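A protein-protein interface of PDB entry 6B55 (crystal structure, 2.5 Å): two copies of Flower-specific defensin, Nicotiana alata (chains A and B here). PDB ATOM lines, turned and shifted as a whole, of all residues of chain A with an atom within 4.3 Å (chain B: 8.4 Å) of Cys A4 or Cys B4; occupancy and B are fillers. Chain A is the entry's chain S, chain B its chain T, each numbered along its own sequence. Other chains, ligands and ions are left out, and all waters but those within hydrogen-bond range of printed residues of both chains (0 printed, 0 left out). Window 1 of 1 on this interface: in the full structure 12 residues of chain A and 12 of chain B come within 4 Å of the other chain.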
ATOM      1  N   GLU A   3      31.669 -13.349   9.436  1.00  0.00           N
ATOM      2  CA  GLU A   3      30.218 -13.388   9.551  1.00  0.00           C
ATOM      3  C   GLU A   3      29.639 -14.195   8.399  1.00  0.00           C
ATOM      4  O   GLU A   3      29.966 -13.949   7.233  1.00  0.00           O
ATOM      5  CB  GLU A   3      29.617 -11.974   9.580  1.00  0.00           C
ATOM      6  CG  GLU A   3      30.023 -11.070   8.425  1.00  0.00           C
ATOM      7  CD  GLU A   3      29.426  -9.679   8.540  1.00  0.00           C
ATOM      8  OE1 GLU A   3      28.910  -9.339   9.625  1.00  0.00           O
ATOM      9  OE2 GLU A   3      29.470  -8.927   7.543  1.00  0.00           O
ATOM     10  N   CYS A   4      28.795 -15.166   8.733  1.00  0.00           N
ATOM     11  CA  CYS A   4      28.094 -15.950   7.727  1.00  0.00           C
ATOM     12  C   CYS A   4      26.837 -15.208   7.293  1.00  0.00           C
ATOM     13  O   CYS A   4      26.050 -14.756   8.132  1.00  0.00           O
ATOM     14  CB  CYS A   4      27.756 -17.337   8.275  1.00  0.00           C
ATOM     15  SG  CYS A   4      29.113 -18.527   8.089  1.00  0.00           S
ATOM     16  N   LYS A   5      26.653 -15.076   5.982  1.00  0.00           N
ATOM     17  CA  LYS A   5      25.654 -14.185   5.411  1.00  0.00           C
ATOM     18  C   LYS A   5      24.665 -14.961   4.553  1.00  0.00           C
ATOM     19  O   LYS A   5      25.035 -15.917   3.864  1.00  0.00           O
ATOM     20  CB  LYS A   5      26.327 -13.090   4.571  1.00  0.00           C
ATOM     21  CG  LYS A   5      25.371 -12.075   3.967  1.00  0.00           C
ATOM     22  CD  LYS A   5      26.106 -11.102   3.058  1.00  0.00           C
ATOM     23  CE  LYS A   5      26.799 -11.831   1.917  1.00  0.00           C
ATOM     24  NZ  LYS A   5      27.548 -10.898   1.031  1.00  0.00           N
ATOM     25  N   THR A   6      23.402 -14.539   4.603  1.00  0.00           N
ATOM     26  CA  THR A   6      22.362 -15.061   3.729  1.00  0.00           C
ATOM     27  C   THR A   6      21.287 -13.994   3.576  1.00  0.00           C
ATOM     28  O   THR A   6      21.123 -13.125   4.436  1.00  0.00           O
ATOM     29  CB  THR A   6      21.755 -16.362   4.267  1.00  0.00           C
ATOM     30  OG1 THR A   6      20.823 -16.887   3.313  1.00  0.00           O
ATOM     31  CG2 THR A   6      21.035 -16.112   5.580  1.00  0.00           C
ATOM     32  N   PHE A  30      19.038 -14.489  13.651  1.00  0.00           N
ATOM     33  CA  PHE A  30      20.386 -14.030  13.355  1.00  0.00           C
ATOM     34  C   PHE A  30      20.786 -12.945  14.354  1.00  0.00           C
ATOM     35  O   PHE A  30      20.043 -12.611  15.278  1.00  0.00           O
ATOM     36  CB  PHE A  30      20.481 -13.525  11.914  1.00  0.00           C
ATOM     37  CG  PHE A  30      20.513 -14.623  10.891  1.00  0.00           C
ATOM     38  CD1 PHE A  30      21.710 -15.018  10.318  1.00  0.00           C
ATOM     39  CD2 PHE A  30      19.349 -15.265  10.505  1.00  0.00           C
ATOM     40  CE1 PHE A  30      21.745 -16.031   9.377  1.00  0.00           C
ATOM     41  CE2 PHE A  30      19.377 -16.278   9.566  1.00  0.00           C
ATOM     42  CZ  PHE A  30      20.577 -16.662   9.002  1.00  0.00           C
ATOM     43  N   CYS A  44      21.083 -10.872   6.111  1.00  0.00           N
ATOM     44  CA  CYS A  44      21.273 -11.241   7.505  1.00  0.00           C
ATOM     45  C   CYS A  44      22.657 -11.841   7.722  1.00  0.00           C
ATOM     46  O   CYS A  44      23.226 -12.483   6.835  1.00  0.00           O
ATOM     47  CB  CYS A  44      20.201 -12.235   7.949  1.00  0.00           C
ATOM     48  SG  CYS A  44      18.522 -11.616   7.769  1.00  0.00           S
ATOM     49  N   THR A  45      23.199 -11.620   8.918  1.00  0.00           N
ATOM     50  CA  THR A  45      24.517 -12.116   9.282  1.00  0.00           C
ATOM     51  C   THR A  45      24.471 -12.754  10.663  1.00  0.00           C
ATOM     52  O   THR A  45      23.638 -12.403  11.503  1.00  0.00           O
ATOM     53  CB  THR A  45      25.575 -10.998   9.276  1.00  0.00           C
ATOM     54  OG1 THR A  45      25.198  -9.973  10.204  1.00  0.00           O
ATOM     55  CG2 THR A  45      25.719 -10.397   7.884  1.00  0.00           C
ATOM     56  N   LYS A  46      25.380 -13.701  10.884  1.00  0.00           N
ATOM     57  CA  LYS A  46      25.565 -14.330  12.184  1.00  0.00           C
ATOM     58  C   LYS A  46      26.954 -14.945  12.212  1.00  0.00           C
ATOM     59  O   LYS A  46      27.501 -15.269  11.150  1.00  0.00           O
ATOM     60  CB  LYS A  46      24.493 -15.398  12.452  1.00  0.00           C
ATOM     61  CG  LYS A  46      24.628 -16.665  11.621  1.00  0.00           C
ATOM     62  CD  LYS A  46      23.555 -17.677  11.997  1.00  0.00           C
ATOM     63  CE  LYS A  46      23.707 -18.968  11.212  1.00  0.00           C
ATOM     64  NZ  LYS A  46      25.003 -19.643  11.500  1.00  0.00           N
ATOM     65  N   CYS A  48      29.930 -17.435  12.145  1.00  0.00           N
ATOM     66  CA  CYS A  48      30.082 -18.780  11.603  1.00  0.00           C
ATOM     67  C   CYS A  48      30.559 -19.743  12.687  1.00  0.00           C
ATOM     68  O   CYS A  48      31.034 -19.323  13.742  1.00  0.00           O
ATOM     69  CB  CYS A  48      31.064 -18.793  10.431  1.00  0.00           C
ATOM     70  SG  CYS A  48      30.684 -17.672   9.057  1.00  0.00           S
ATOM     71  OXT CYS A  48      30.487 -20.962  12.530  1.00  0.00           O
ATOM     72  N   ALA B   1      16.798 -26.153   2.568  1.00  0.00           N
ATOM     73  CA  ALA B   1      17.767 -25.809   3.602  1.00  0.00           C
ATOM     74  C   ALA B   1      18.397 -24.446   3.330  1.00  0.00           C
ATOM     75  O   ALA B   1      18.910 -24.194   2.240  1.00  0.00           O
ATOM     76  CB  ALA B   1      18.843 -26.882   3.698  1.00  0.00           C
ATOM     77  N   ARG B   2      18.353 -23.572   4.332  1.00  0.00           N
ATOM     78  CA  ARG B   2      18.914 -22.237   4.187  1.00  0.00           C
ATOM     79  C   ARG B   2      20.437 -22.302   4.166  1.00  0.00           C
ATOM     80  O   ARG B   2      21.054 -23.025   4.953  1.00  0.00           O
ATOM     81  CB  ARG B   2      18.433 -21.341   5.327  1.00  0.00           C
ATOM     82  CG  ARG B   2      18.422 -19.861   5.000  1.00  0.00           C
ATOM     83  CD  ARG B   2      17.655 -19.083   6.056  1.00  0.00           C
ATOM     84  NE  ARG B   2      17.491 -17.678   5.696  1.00  0.00           N
ATOM     85  CZ  ARG B   2      16.779 -16.808   6.404  1.00  0.00           C
ATOM     86  NH1 ARG B   2      16.161 -17.197   7.511  1.00  0.00           N
ATOM     87  NH2 ARG B   2      16.682 -15.547   6.004  1.00  0.00           N
ATOM     88  N   GLU B   3      21.042 -21.540   3.259  1.00  0.00           N
ATOM     89  CA  GLU B   3      22.478 -21.596   3.011  1.00  0.00           C
ATOM     90  C   GLU B   3      23.129 -20.290   3.446  1.00  0.00           C
ATOM     91  O   GLU B   3      22.740 -19.213   2.983  1.00  0.00           O
ATOM     92  CB  GLU B   3      22.763 -21.870   1.534  1.00  0.00           C
ATOM     93  CG  GLU B   3      24.222 -21.710   1.143  1.00  0.00           C
ATOM     94  CD  GLU B   3      24.500 -22.181  -0.273  1.00  0.00           C
ATOM     95  OE1 GLU B   3      24.511 -23.410  -0.501  1.00  0.00           O
ATOM     96  OE2 GLU B   3      24.698 -21.323  -1.159  1.00  0.00           O
ATOM     97  N   CYS B   4      24.119 -20.392   4.329  1.00  0.00           N
ATOM     98  CA  CYS B   4      24.924 -19.262   4.764  1.00  0.00           C
ATOM     99  C   CYS B   4      26.236 -19.230   3.988  1.00  0.00           C
ATOM    100  O   CYS B   4      26.731 -20.262   3.532  1.00  0.00           O
ATOM    101  CB  CYS B   4      25.191 -19.334   6.270  1.00  0.00           C
ATOM    102  SG  CYS B   4      23.846 -18.656   7.269  1.00  0.00           S
ATOM    103  N   LYS B   5      26.797 -18.031   3.840  1.00  0.00           N
ATOM    104  CA  LYS B   5      27.925 -17.828   2.943  1.00  0.00           C
ATOM    105  C   LYS B   5      28.913 -16.834   3.535  1.00  0.00           C
ATOM    106  O   LYS B   5      28.517 -15.877   4.207  1.00  0.00           O
ATOM    107  CB  LYS B   5      27.443 -17.335   1.570  1.00  0.00           C
ATOM    108  CG  LYS B   5      28.542 -17.116   0.548  1.00  0.00           C
ATOM    109  CD  LYS B   5      27.972 -16.565  -0.748  1.00  0.00           C
ATOM    110  CE  LYS B   5      27.203 -15.278  -0.504  1.00  0.00           C
ATOM    111  NZ  LYS B   5      26.628 -14.732  -1.762  1.00  0.00           N
ATOM    112  N   THR B   6      30.199 -17.073   3.281  1.00  0.00           N
ATOM    113  CA  THR B   6      31.267 -16.157   3.661  1.00  0.00           C
ATOM    114  C   THR B   6      32.490 -16.473   2.813  1.00  0.00           C
ATOM    115  O   THR B   6      32.627 -17.576   2.279  1.00  0.00           O
ATOM    116  CB  THR B   6      31.605 -16.260   5.152  1.00  0.00           C
ATOM    117  OG1 THR B   6      32.694 -15.378   5.458  1.00  0.00           O
ATOM    118  CG2 THR B   6      32.003 -17.680   5.510  1.00  0.00           C
ATOM    119  N   GLU B   7      33.376 -15.489   2.693  1.00  0.00           N
ATOM    120  CA  GLU B   7      34.588 -15.681   1.907  1.00  0.00           C
ATOM    121  C   GLU B   7      35.588 -16.549   2.666  1.00  0.00           C
ATOM    122  O   GLU B   7      35.694 -16.490   3.894  1.00  0.00           O
ATOM    123  CB  GLU B   7      35.223 -14.336   1.550  1.00  0.00           C
ATOM    124  CG  GLU B   7      36.401 -14.450   0.586  1.00  0.00           C
ATOM    125  CD  GLU B   7      36.950 -13.103   0.159  1.00  0.00           C
ATOM    126  OE1 GLU B   7      36.315 -12.073   0.468  1.00  0.00           O
ATOM    127  OE2 GLU B   7      38.023 -13.075  -0.481  1.00  0.00           O
ATOM    128  N   LYS B  29      35.811 -26.176   7.788  1.00  0.00           N
ATOM    129  CA  LYS B  29      34.594 -26.658   8.445  1.00  0.00           C
ATOM    130  C   LYS B  29      33.335 -26.074   7.801  1.00  0.00           C
ATOM    131  O   LYS B  29      32.410 -25.643   8.490  1.00  0.00           O
ATOM    132  CB  LYS B  29      34.617 -26.380   9.951  1.00  0.00           C
ATOM    133  CG  LYS B  29      35.872 -26.874  10.656  1.00  0.00           C
ATOM    134  CD  LYS B  29      36.170 -28.329  10.323  1.00  0.00           C
ATOM    135  CE  LYS B  29      37.452 -28.795  10.994  1.00  0.00           C
ATOM    136  NZ  LYS B  29      38.619 -27.954  10.608  1.00  0.00           N
ATOM    137  N   PHE B  30      33.303 -26.059   6.474  1.00  0.00           N
ATOM    138  CA  PHE B  30      32.113 -25.745   5.694  1.00  0.00           C
ATOM    139  C   PHE B  30      31.742 -26.964   4.853  1.00  0.00           C
ATOM    140  O   PHE B  30      32.440 -27.980   4.853  1.00  0.00           O
ATOM    141  CB  PHE B  30      32.335 -24.512   4.813  1.00  0.00           C
ATOM    142  CG  PHE B  30      32.418 -23.223   5.581  1.00  0.00           C
ATOM    143  CD1 PHE B  30      33.615 -22.810   6.141  1.00  0.00           C
ATOM    144  CD2 PHE B  30      31.298 -22.419   5.736  1.00  0.00           C
ATOM    145  CE1 PHE B  30      33.695 -21.623   6.847  1.00  0.00           C
ATOM    146  CE2 PHE B  30      31.371 -21.230   6.439  1.00  0.00           C
ATOM    147  CZ  PHE B  30      32.570 -20.832   6.997  1.00  0.00           C
ATOM    148  N   THR B  31      30.628 -26.863   4.130  1.00  0.00           N
ATOM    149  CA  THR B  31      30.159 -27.979   3.318  1.00  0.00           C
ATOM    150  C   THR B  31      30.583 -27.891   1.859  1.00  0.00           C
ATOM    151  O   THR B  31      30.776 -28.933   1.224  1.00  0.00           O
ATOM    152  CB  THR B  31      28.630 -28.090   3.377  1.00  0.00           C
ATOM    153  OG1 THR B  31      28.041 -26.887   2.869  1.00  0.00           O
ATOM    154  CG2 THR B  31      28.169 -28.316   4.805  1.00  0.00           C
ATOM    155  N   ASP B  32      30.741 -26.687   1.315  1.00  0.00           N
ATOM    156  CA  ASP B  32      31.036 -26.534  -0.102  1.00  0.00           C
ATOM    157  C   ASP B  32      31.596 -25.139  -0.344  1.00  0.00           C
ATOM    158  O   ASP B  32      31.495 -24.251   0.507  1.00  0.00           O
ATOM    159  CB  ASP B  32      29.784 -26.793  -0.953  1.00  0.00           C
ATOM    160  CG  ASP B  32      30.075 -26.821  -2.439  1.00  0.00           C
ATOM    161  OD1 ASP B  32      29.742 -25.835  -3.130  1.00  0.00           O
ATOM    162  OD2 ASP B  32      30.653 -27.822  -2.913  1.00  0.00           O
ATOM    163  N   HIS B  34      32.572 -22.153  -3.756  1.00  0.00           N
ATOM    164  CA  HIS B  34      32.413 -21.749  -5.146  1.00  0.00           C
ATOM    165  C   HIS B  34      32.987 -20.352  -5.320  1.00  0.00           C
ATOM    166  O   HIS B  34      33.196 -19.621  -4.349  1.00  0.00           O
ATOM    167  CB  HIS B  34      30.945 -21.790  -5.589  1.00  0.00           C
ATOM    168  CG  HIS B  34      30.080 -20.776  -4.907  1.00  0.00           C
ATOM    169  ND1 HIS B  34      29.480 -21.008  -3.689  1.00  0.00           N
ATOM    170  CD2 HIS B  34      29.714 -19.526  -5.276  1.00  0.00           C
ATOM    171  CE1 HIS B  34      28.781 -19.944  -3.336  1.00  0.00           C
ATOM    172  NE2 HIS B  34      28.906 -19.030  -4.283  1.00  0.00           N
ATOM    173  N   LEU B  43      34.164 -18.465  -2.051  1.00  0.00           N
ATOM    174  CA  LEU B  43      33.121 -18.288  -1.050  1.00  0.00           C
ATOM    175  C   LEU B  43      32.723 -19.645  -0.490  1.00  0.00           C
ATOM    176  O   LEU B  43      32.416 -20.569  -1.251  1.00  0.00           O
ATOM    177  CB  LEU B  43      31.903 -17.580  -1.648  1.00  0.00           C
ATOM    178  CG  LEU B  43      32.169 -16.227  -2.309  1.00  0.00           C
ATOM    179  CD1 LEU B  43      30.879 -15.630  -2.854  1.00  0.00           C
ATOM    180  CD2 LEU B  43      32.835 -15.269  -1.333  1.00  0.00           C
ATOM    181  N   CYS B  44      32.727 -19.759   0.834  1.00  0.00           N
ATOM    182  CA  CYS B  44      32.376 -20.991   1.521  1.00  0.00           C
ATOM    183  C   CYS B  44      30.911 -20.967   1.935  1.00  0.00           C
ATOM    184  O   CYS B  44      30.365 -19.922   2.295  1.00  0.00           O
ATOM    185  CB  CYS B  44      33.265 -21.197   2.747  1.00  0.00           C
ATOM    186  SG  CYS B  44      35.018 -21.274   2.339  1.00  0.00           S
ATOM    187  N   THR B  45      30.275 -22.137   1.875  1.00  0.00           N
ATOM    188  CA  THR B  45      28.854 -22.265   2.156  1.00  0.00           C
ATOM    189  C   THR B  45      28.604 -23.433   3.102  1.00  0.00           C
ATOM    190  O   THR B  45      29.333 -24.430   3.096  1.00  0.00           O
ATOM    191  CB  THR B  45      28.038 -22.466   0.866  1.00  0.00           C
ATOM    192  OG1 THR B  45      28.576 -23.568   0.122  1.00  0.00           O
ATOM    193  CG2 THR B  45      28.071 -21.209   0.007  1.00  0.00           C
ATOM    194  N   LYS B  46      27.559 -23.290   3.913  1.00  0.00           N
ATOM    195  CA  LYS B  46      27.126 -24.321   4.845  1.00  0.00           C
ATOM    196  C   LYS B  46      25.713 -23.984   5.301  1.00  0.00           C
ATOM    197  O   LYS B  46      25.279 -22.832   5.177  1.00  0.00           O
ATOM    198  CB  LYS B  46      28.077 -24.423   6.050  1.00  0.00           C
ATOM    199  CG  LYS B  46      27.983 -23.271   7.029  1.00  0.00           C
ATOM    200  CD  LYS B  46      28.837 -23.534   8.258  1.00  0.00           C
ATOM    201  CE  LYS B  46      28.705 -22.418   9.278  1.00  0.00           C
ATOM    202  NZ  LYS B  46      29.473 -22.715  10.518  1.00  0.00           N
ATOM    203  N   PRO B  47      24.964 -24.962   5.808  1.00  0.00           N
ATOM    204  CA  PRO B  47      23.613 -24.669   6.297  1.00  0.00           C
ATOM    205  C   PRO B  47      23.649 -23.714   7.482  1.00  0.00           C
ATOM    206  O   PRO B  47      24.514 -23.809   8.355  1.00  0.00           O
ATOM    207  CB  PRO B  47      23.072 -26.046   6.701  1.00  0.00           C
ATOM    208  CG  PRO B  47      23.888 -27.020   5.915  1.00  0.00           C
ATOM    209  CD  PRO B  47      25.250 -26.409   5.825  1.00  0.00           C
ATOM    210  N   CYS B  48      22.697 -22.787   7.502  1.00  0.00           N
ATOM    211  CA  CYS B  48      22.595 -21.819   8.589  1.00  0.00           C
ATOM    212  C   CYS B  48      22.042 -22.473   9.851  1.00  0.00           C
ATOM    213  O   CYS B  48      21.755 -23.671   9.873  1.00  0.00           O
ATOM    214  CB  CYS B  48      21.707 -20.639   8.190  1.00  0.00           C
ATOM    215  SG  CYS B  48      22.209 -19.725   6.710  1.00  0.00           S
ATOM    216  OXT CYS B  48      21.860 -21.817  10.876  1.00  0.00           O
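The backbone NH (N) of Lys A5 sits at hydrogen-bond distance from the backbone carbonyl oxygen (O) of Lys B5.
The side-chain hydroxyl (OG1) of Thr A6 sits at hydrogen-bond distance from the backbone carbonyl oxygen (O) of Glu B3, 3.0 Å away.
NZ of Lys A46 lies within salt-bridge range of OXT of Cys B48 (3.9 Å).
OXT of Cys A48 is in salt-bridge range of NZ of Lys B46 (2.9 Å).
The backbone NH (N) of Cys A4 lies within hydrogen-bond range of the backbone carbonyl oxygen (O) of Lys A46 (2.7 Å).
The side-chain sulfur (SG) of Cys A4 forms a disulfide with the side-chain sulfur (SG) of Cys A48 (2.0 Å).
The backbone carbonyl oxygen of Thr A6 sits at hydrogen-bond distance from the backbone NH of Cys A44 (2.8 Å).
O of Lys B46 sits at hydrogen-bond distance from N of Cys B4, at 2.8 Å.
The side-chain sulfur (SG) of Cys B4 is disulfide-bonded to the side-chain sulfur (SG) of Cys B48, 2.0 Å away.
The backbone NH (N) of Cys B44 lies within hydrogen-bond range of the backbone carbonyl oxygen (O) of Thr B6, at 2.6 Å.
Among the printed residues, pairs that only touch across the chains: Lys A5 with Cys B4 (3.5 Å), Glu A3 with Thr B6 (3.5 Å), Cys A4 with Lys B5 (3.5 Å), Cys A48 with Thr B6 (3.8 Å), Cys A4 with Cys B4 (3.8 Å), Glu A3 with Lys B5 (3.9 Å), Thr A6 with Arg B2 (3.9 Å), Cys A4 with Phe B30 (3.9 Å), Phe A30 with Arg B2 (3.9 Å), Lys A46 with Cys B4 (3.96 Å), Thr A6 with Cys B48 (3.96 Å), Cys A4 with Thr B6 (3.96 Å) and Phe A30 with Cys B4 (3.97 Å).
Of chain A, only Cys A4, Lys A5, Phe A30 and Lys A46 come within 4 Å of Cys B4.
Printed residues of chain B within 4 Å of Glu A3: Lys B5 (3.9 Å) and Thr B6 (3.5 Å).
Of the printed residues of chain B, Phe A30 touches Arg B2 and Cys B4.
Of the printed residues of chain A, Cys B48 touches Thr A6 and Lys A46.
Of the printed residues of chain A, Arg B2 touches Thr A6 (3.9 Å) and Phe A30 (3.9 Å).
His B34 touches none of the printed residues of chain A.
The nearest printed residue of chain A that does not touch Glu B3 is Lys A5 (4.1 Å).
Hydrophobic or aromatic side chains of chain B that line the printed part of chain A: Phe B30.
Of the 9 printed residues of chain A, 7 touch a printed residue of chain B.
Among the printed residues, 17 pairs touch across the chains.
Among the printed residues, no Asp or Glu carboxylate lies within 4 Å of a Lys or Arg side-chain nitrogen of the other chain.
Cys B4 touches its own counterpart, Cys A4.
Cys A4 touches Phe B30, and with the chains exchanged Phe A30 touches Cys B4.
Thr A6 touches Cys B48, and with the chains exchanged Cys A48 touches Thr B6.
Lys A46 touches Cys B4, but with the chains exchanged Cys A4 does not touch Lys B46 (4.1 Å).
Positions printed for both chains: 3, 4, 5, 6, 30, 44, 45, 46 and 48.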
